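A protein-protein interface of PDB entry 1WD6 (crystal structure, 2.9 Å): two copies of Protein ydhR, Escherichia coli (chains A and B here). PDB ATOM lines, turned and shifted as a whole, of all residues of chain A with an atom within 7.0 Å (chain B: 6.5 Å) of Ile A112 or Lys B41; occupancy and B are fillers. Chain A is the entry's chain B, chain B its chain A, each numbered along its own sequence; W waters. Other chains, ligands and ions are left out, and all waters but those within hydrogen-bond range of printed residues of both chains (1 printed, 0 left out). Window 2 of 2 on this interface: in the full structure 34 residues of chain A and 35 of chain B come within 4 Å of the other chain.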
ATOM      1  N   GLU A 107     -35.002  19.228  28.925  1.00  0.00           N
ATOM      2  CA  GLU A 107     -35.672  18.710  27.739  1.00  0.00           C
ATOM      3  C   GLU A 107     -35.523  19.537  26.462  1.00  0.00           C
ATOM      4  O   GLU A 107     -35.170  19.002  25.410  1.00  0.00           O
ATOM      5  CB  GLU A 107     -37.161  18.484  28.026  1.00  0.00           C
ATOM      6  CG  GLU A 107     -37.608  17.023  27.940  1.00  0.00           C
ATOM      7  CD  GLU A 107     -37.207  16.196  29.163  1.00  0.00           C
ATOM      8  OE1 GLU A 107     -37.635  16.535  30.291  1.00  0.00           O
ATOM      9  OE2 GLU A 107     -36.468  15.201  28.997  1.00  0.00           O
ATOM     10  N   PRO A 108     -35.786  20.852  26.534  1.00  0.00           N
ATOM     11  CA  PRO A 108     -35.668  21.702  25.343  1.00  0.00           C
ATOM     12  C   PRO A 108     -34.343  21.528  24.576  1.00  0.00           C
ATOM     13  O   PRO A 108     -34.346  21.352  23.357  1.00  0.00           O
ATOM     14  CB  PRO A 108     -35.830  23.109  25.911  1.00  0.00           C
ATOM     15  CG  PRO A 108     -36.694  22.898  27.115  1.00  0.00           C
ATOM     16  CD  PRO A 108     -36.096  21.661  27.727  1.00  0.00           C
ATOM     17  N   LEU A 109     -33.219  21.579  25.295  1.00  0.00           N
ATOM     18  CA  LEU A 109     -31.899  21.432  24.685  1.00  0.00           C
ATOM     19  C   LEU A 109     -31.649  19.996  24.250  1.00  0.00           C
ATOM     20  O   LEU A 109     -31.103  19.745  23.174  1.00  0.00           O
ATOM     21  CB  LEU A 109     -30.812  21.877  25.666  1.00  0.00           C
ATOM     22  CG  LEU A 109     -30.891  23.342  26.116  1.00  0.00           C
ATOM     23  CD1 LEU A 109     -29.925  23.592  27.256  1.00  0.00           C
ATOM     24  CD2 LEU A 109     -30.588  24.254  24.945  1.00  0.00           C
ATOM     25  N   SER A 110     -32.050  19.046  25.085  1.00  0.00           N
ATOM     26  CA  SER A 110     -31.866  17.641  24.753  1.00  0.00           C
ATOM     27  C   SER A 110     -32.630  17.304  23.479  1.00  0.00           C
ATOM     28  O   SER A 110     -32.198  16.452  22.697  1.00  0.00           O
ATOM     29  CB  SER A 110     -32.333  16.771  25.910  1.00  0.00           C
ATOM     30  OG  SER A 110     -31.552  17.044  27.059  1.00  0.00           O
ATOM     31  N   GLN A 111     -33.759  17.981  23.270  1.00  0.00           N
ATOM     32  CA  GLN A 111     -34.570  17.780  22.069  1.00  0.00           C
ATOM     33  C   GLN A 111     -33.725  18.114  20.842  1.00  0.00           C
ATOM     34  O   GLN A 111     -33.647  17.328  19.899  1.00  0.00           O
ATOM     35  CB  GLN A 111     -35.803  18.690  22.073  1.00  0.00           C
ATOM     36  CG  GLN A 111     -36.776  18.468  23.223  1.00  0.00           C
ATOM     37  CD  GLN A 111     -37.482  17.120  23.160  1.00  0.00           C
ATOM     38  OE1 GLN A 111     -38.194  16.821  22.192  1.00  0.00           O
ATOM     39  NE2 GLN A 111     -37.291  16.300  24.197  1.00  0.00           N
ATOM     40  N   ILE A 112     -33.090  19.285  20.862  1.00  0.00           N
ATOM     41  CA  ILE A 112     -32.251  19.719  19.752  1.00  0.00           C
ATOM     42  C   ILE A 112     -31.182  18.680  19.422  1.00  0.00           C
ATOM     43  O   ILE A 112     -30.944  18.368  18.251  1.00  0.00           O
ATOM     44  CB  ILE A 112     -31.536  21.058  20.070  1.00  0.00           C
ATOM     45  CG1 ILE A 112     -32.562  22.153  20.337  1.00  0.00           C
ATOM     46  CG2 ILE A 112     -30.641  21.469  18.909  1.00  0.00           C
ATOM     47  CD1 ILE A 112     -31.943  23.473  20.726  1.00  0.00           C
ATOM     48  N   ASN A 113     -30.548  18.132  20.454  1.00  0.00           N
ATOM     49  CA  ASN A 113     -29.485  17.161  20.246  1.00  0.00           C
ATOM     50  C   ASN A 113     -29.902  15.707  20.134  1.00  0.00           C
ATOM     51  O   ASN A 113     -29.382  14.839  20.834  1.00  0.00           O
ATOM     52  CB  ASN A 113     -28.446  17.340  21.331  1.00  0.00           C
ATOM     53  CG  ASN A 113     -27.746  18.660  21.217  1.00  0.00           C
ATOM     54  OD1 ASN A 113     -27.654  19.415  22.180  1.00  0.00           O
ATOM     55  ND2 ASN A 113     -27.248  18.954  20.023  1.00  0.00           N
ATOM     56  N   GLN A 114     -30.829  15.459  19.212  1.00  0.00           N
ATOM     57  CA  GLN A 114     -31.358  14.131  18.927  1.00  0.00           C
ATOM     58  C   GLN A 114     -32.312  13.703  20.023  1.00  0.00           C
ATOM     59  O   GLN A 114     -33.508  13.519  19.711  1.00  0.00           O
ATOM     60  CB  GLN A 114     -30.214  13.124  18.794  1.00  0.00           C
ATOM     61  CG  GLN A 114     -30.498  11.981  17.834  1.00  0.00           C
ATOM     62  CD  GLN A 114     -31.372  10.899  18.430  1.00  0.00           C
ATOM     63  OE1 GLN A 114     -31.865  10.025  17.712  1.00  0.00           O
ATOM     64  NE2 GLN A 114     -31.559  10.937  19.747  1.00  0.00           N
ATOM     65  N   MET B  36     -31.851  28.441  30.773  1.00  0.00           N
ATOM     66  CA  MET B  36     -30.683  27.774  30.216  1.00  0.00           C
ATOM     67  C   MET B  36     -30.996  27.303  28.803  1.00  0.00           C
ATOM     68  O   MET B  36     -30.162  27.406  27.905  1.00  0.00           O
ATOM     69  CB  MET B  36     -30.291  26.577  31.079  1.00  0.00           C
ATOM     70  CG  MET B  36     -29.025  25.862  30.608  1.00  0.00           C
ATOM     71  SD  MET B  36     -28.817  24.091  31.375  1.00  0.00           S
ATOM     72  CE  MET B  36     -27.979  24.559  33.054  1.00  0.00           C
ATOM     73  N   ALA B  37     -32.202  26.780  28.613  1.00  0.00           N
ATOM     74  CA  ALA B  37     -32.633  26.299  27.307  1.00  0.00           C
ATOM     75  C   ALA B  37     -32.569  27.435  26.283  1.00  0.00           C
ATOM     76  O   ALA B  37     -32.147  27.243  25.142  1.00  0.00           O
ATOM     77  CB  ALA B  37     -34.051  25.754  27.402  1.00  0.00           C
ATOM     78  N   GLU B  38     -32.993  28.622  26.704  1.00  0.00           N
ATOM     79  CA  GLU B  38     -32.980  29.801  25.845  1.00  0.00           C
ATOM     80  C   GLU B  38     -31.539  30.231  25.596  1.00  0.00           C
ATOM     81  O   GLU B  38     -31.077  30.290  24.462  1.00  0.00           O
ATOM     82  CB  GLU B  38     -33.735  30.938  26.525  1.00  0.00           C
ATOM     83  CG  GLU B  38     -33.729  32.254  25.764  1.00  0.00           C
ATOM     84  CD  GLU B  38     -34.228  33.421  26.614  1.00  0.00           C
ATOM     85  OE1 GLU B  38     -34.399  34.532  26.068  1.00  0.00           O
ATOM     86  OE2 GLU B  38     -34.443  33.227  27.835  1.00  0.00           O
ATOM     87  N   GLN B  39     -30.835  30.518  26.682  1.00  0.00           N
ATOM     88  CA  GLN B  39     -29.453  30.962  26.637  1.00  0.00           C
ATOM     89  C   GLN B  39     -28.502  30.072  25.842  1.00  0.00           C
ATOM     90  O   GLN B  39     -27.809  30.538  24.941  1.00  0.00           O
ATOM     91  CB  GLN B  39     -28.925  31.102  28.061  1.00  0.00           C
ATOM     92  CG  GLN B  39     -27.583  31.786  28.154  1.00  0.00           C
ATOM     93  CD  GLN B  39     -27.652  33.224  27.702  1.00  0.00           C
ATOM     94  OE1 GLN B  39     -28.494  33.987  28.174  1.00  0.00           O
ATOM     95  NE2 GLN B  39     -26.768  33.606  26.786  1.00  0.00           N
ATOM     96  N   LEU B  40     -28.470  28.787  26.166  1.00  0.00           N
ATOM     97  CA  LEU B  40     -27.549  27.883  25.499  1.00  0.00           C
ATOM     98  C   LEU B  40     -28.042  27.242  24.214  1.00  0.00           C
ATOM     99  O   LEU B  40     -27.335  26.425  23.628  1.00  0.00           O
ATOM    100  CB  LEU B  40     -27.106  26.799  26.480  1.00  0.00           C
ATOM    101  CG  LEU B  40     -26.518  27.290  27.804  1.00  0.00           C
ATOM    102  CD1 LEU B  40     -26.112  26.095  28.622  1.00  0.00           C
ATOM    103  CD2 LEU B  40     -25.323  28.181  27.565  1.00  0.00           C
ATOM    104  N   LYS B  41     -29.235  27.614  23.763  1.00  0.00           N
ATOM    105  CA  LYS B  41     -29.781  27.037  22.535  1.00  0.00           C
ATOM    106  C   LYS B  41     -28.817  27.052  21.343  1.00  0.00           C
ATOM    107  O   LYS B  41     -28.748  26.084  20.576  1.00  0.00           O
ATOM    108  CB  LYS B  41     -31.063  27.742  22.125  1.00  0.00           C
ATOM    109  CG  LYS B  41     -31.570  27.219  20.802  1.00  0.00           C
ATOM    110  CD  LYS B  41     -32.845  27.887  20.368  1.00  0.00           C
ATOM    111  CE  LYS B  41     -33.344  27.241  19.094  1.00  0.00           C
ATOM    112  NZ  LYS B  41     -34.684  27.762  18.716  1.00  0.00           N
ATOM    113  N   PRO B  42     -28.081  28.162  21.152  1.00  0.00           N
ATOM    114  CA  PRO B  42     -27.133  28.248  20.037  1.00  0.00           C
ATOM    115  C   PRO B  42     -26.120  27.121  20.146  1.00  0.00           C
ATOM    116  O   PRO B  42     -25.887  26.368  19.198  1.00  0.00           O
ATOM    117  CB  PRO B  42     -26.479  29.607  20.248  1.00  0.00           C
ATOM    118  CG  PRO B  42     -27.556  30.405  20.898  1.00  0.00           C
ATOM    119  CD  PRO B  42     -28.125  29.435  21.894  1.00  0.00           C
ATOM    120  N   LEU B  43     -25.532  27.019  21.333  1.00  0.00           N
ATOM    121  CA  LEU B  43     -24.522  26.019  21.658  1.00  0.00           C
ATOM    122  C   LEU B  43     -24.967  24.590  21.348  1.00  0.00           C
ATOM    123  O   LEU B  43     -24.180  23.776  20.883  1.00  0.00           O
ATOM    124  CB  LEU B  43     -24.181  26.149  23.138  1.00  0.00           C
ATOM    125  CG  LEU B  43     -22.734  25.929  23.552  1.00  0.00           C
ATOM    126  CD1 LEU B  43     -22.546  26.499  24.943  1.00  0.00           C
ATOM    127  CD2 LEU B  43     -22.386  24.453  23.499  1.00  0.00           C
ATOM    128  N   ALA B  44     -26.234  24.294  21.611  1.00  0.00           N
ATOM    129  CA  ALA B  44     -26.792  22.968  21.371  1.00  0.00           C
ATOM    130  C   ALA B  44     -26.768  22.585  19.900  1.00  0.00           C
ATOM    131  O   ALA B  44     -26.344  21.488  19.543  1.00  0.00           O
ATOM    132  CB  ALA B  44     -28.219  22.901  21.892  1.00  0.00           C
ATOM    133  N   GLU B  45     -27.228  23.490  19.043  1.00  0.00           N
ATOM    134  CA  GLU B  45     -27.260  23.210  17.617  1.00  0.00           C
ATOM    135  C   GLU B  45     -25.900  23.263  16.944  1.00  0.00           C
ATOM    136  O   GLU B  45     -25.750  22.794  15.815  1.00  0.00           O
ATOM    137  CB  GLU B  45     -28.235  24.148  16.921  1.00  0.00           C
ATOM    138  CG  GLU B  45     -28.328  25.504  17.553  1.00  0.00           C
ATOM    139  CD  GLU B  45     -29.519  26.278  17.041  1.00  0.00           C
ATOM    140  OE1 GLU B  45     -30.661  25.790  17.216  1.00  0.00           O
ATOM    141  OE2 GLU B  45     -29.315  27.369  16.460  1.00  0.00           O
ATOM    142  N   SER B  46     -24.908  23.831  17.624  1.00  0.00           N
ATOM    143  CA  SER B  46     -23.562  23.881  17.065  1.00  0.00           C
ATOM    144  C   SER B  46     -22.890  22.541  17.383  1.00  0.00           C
ATOM    145  O   SER B  46     -21.862  22.186  16.800  1.00  0.00           O
ATOM    146  CB  SER B  46     -22.754  25.005  17.699  1.00  0.00           C
ATOM    147  OG  SER B  46     -22.269  24.618  18.970  1.00  0.00           O
ATOM    148  N   ASN B  48     -24.590  19.593  17.156  1.00  0.00           N
ATOM    149  CA  ASN B  48     -25.059  18.610  16.179  1.00  0.00           C
ATOM    150  C   ASN B  48     -24.099  18.570  14.998  1.00  0.00           C
ATOM    151  O   ASN B  48     -24.128  17.642  14.189  1.00  0.00           O
ATOM    152  CB  ASN B  48     -26.464  18.945  15.670  1.00  0.00           C
ATOM    153  CG  ASN B  48     -27.529  18.767  16.730  1.00  0.00           C
ATOM    154  OD1 ASN B  48     -27.997  19.734  17.328  1.00  0.00           O
ATOM    155  ND2 ASN B  48     -27.914  17.523  16.978  1.00  0.00           N
ATOM    156  N   PHE B  53     -20.539  12.959  16.455  1.00  0.00           N
ATOM    157  CA  PHE B  53     -21.622  13.183  17.407  1.00  0.00           C
ATOM    158  C   PHE B  53     -22.934  12.494  17.034  1.00  0.00           C
ATOM    159  O   PHE B  53     -23.418  12.632  15.913  1.00  0.00           O
ATOM    160  CB  PHE B  53     -21.876  14.679  17.560  1.00  0.00           C
ATOM    161  CG  PHE B  53     -22.993  15.000  18.494  1.00  0.00           C
ATOM    162  CD1 PHE B  53     -22.845  14.810  19.863  1.00  0.00           C
ATOM    163  CD2 PHE B  53     -24.210  15.449  18.008  1.00  0.00           C
ATOM    164  CE1 PHE B  53     -23.899  15.061  20.737  1.00  0.00           C
ATOM    165  CE2 PHE B  53     -25.270  15.703  18.872  1.00  0.00           C
ATOM    166  CZ  PHE B  53     -25.113  15.507  20.242  1.00  0.00           C
ATOM    167  N   TRP B  58     -28.780  16.777  27.989  1.00  0.00           N
ATOM    168  CA  TRP B  58     -28.302  17.856  28.845  1.00  0.00           C
ATOM    169  C   TRP B  58     -28.765  17.588  30.264  1.00  0.00           C
ATOM    170  O   TRP B  58     -29.947  17.335  30.502  1.00  0.00           O
ATOM    171  CB  TRP B  58     -28.836  19.216  28.373  1.00  0.00           C
ATOM    172  CG  TRP B  58     -28.267  19.687  27.065  1.00  0.00           C
ATOM    173  CD1 TRP B  58     -28.502  19.158  25.831  1.00  0.00           C
ATOM    174  CD2 TRP B  58     -27.373  20.787  26.866  1.00  0.00           C
ATOM    175  NE1 TRP B  58     -27.812  19.860  24.874  1.00  0.00           N
ATOM    176  CE2 TRP B  58     -27.110  20.867  25.481  1.00  0.00           C
ATOM    177  CE3 TRP B  58     -26.770  21.719  27.725  1.00  0.00           C
ATOM    178  CZ2 TRP B  58     -26.266  21.843  24.928  1.00  0.00           C
ATOM    179  CZ3 TRP B  58     -25.929  22.696  27.172  1.00  0.00           C
ATOM    180  CH2 TRP B  58     -25.689  22.745  25.788  1.00  0.00           C
HETATM  181  O   HOH W   1     -29.121  15.226  16.310  1.00  0.00           O
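Among the printed residues, pairs that only touch across the chains: Pro A108 with Ala B37, Leu A109 with Met B36, Leu A109 with Ala B37, Leu A109 with Leu B40, Leu A109 with Lys B41, Leu A109 with Trp B58, Ile A112 with Lys B41, Ile A112 with Ala B44, Ile A112 with Glu B45 and Asn A113 with Phe B53.
Of the 8 printed residues of chain A, 5 touch a printed residue of chain B.
Of the 14 printed residues of chain B, 9 touch a printed residue of chain A.
Hydrophobic or aromatic side chains of chain B that line the printed part of chain A: Ala B37, Ala B44, Phe B53 and Trp B58.
Among the printed residues, no Asp or Glu carboxylate lies within 4 Å of a Lys or Arg side-chain nitrogen of the other chain.
The side-chain amide oxygen (OD1) of Asn B48 lies close to the backbone carbonyl oxygen (O) of Ile A112, 3.4 Å away.
The backbone NH (N) of Trp B58 sits at hydrogen-bond distance from the side-chain hydroxyl (OG) of Ser A110 (2.9 Å).
O of Ala B44 is in hydrogen-bond range of ND2 of Asn A113 (2.7 Å).
ND2 of Asn A113 sits at hydrogen-bond distance from OD1 of Asn B48 (2.9 Å).
The indole nitrogen (NE1) of Trp B58 sits at hydrogen-bond distance from the side-chain amide oxygen (OD1) of Asn A113 (2.7 Å).
Of the printed residues of chain B, Ser A110 touches Trp B58.
Of the printed residues of chain B, Asn A113 touches Ala B44, Asn B48, Phe B53 and Trp B58.
Of the printed residues of chain A, Ala B37 touches Pro A108 (3.5 Å) and Leu A109 (3.4 Å).
Of the printed residues of chain A, Ala B44 touches Ile A112 (3.9 Å) and Asn A113 (2.7 Å).
Of the printed residues of chain A, Phe B53 touches Asn A113 (3.96 Å).
The nearest printed residue of chain A that does not touch Glu B45 is Asn A113 (4.6 Å).
O of Ala B44 lies close to OD1 of Asn B48 (3.3 Å).
No position is printed for both chains.
Of the 15 pairs that touch across the chains among the printed residues, none has its exchanged pair printed and touching as well.
Water W1 lies within hydrogen-bond range of the side-chain amide nitrogen of Asn B48 (2.7 Å) and the backbone NH of Gln A114 (3.4 Å).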
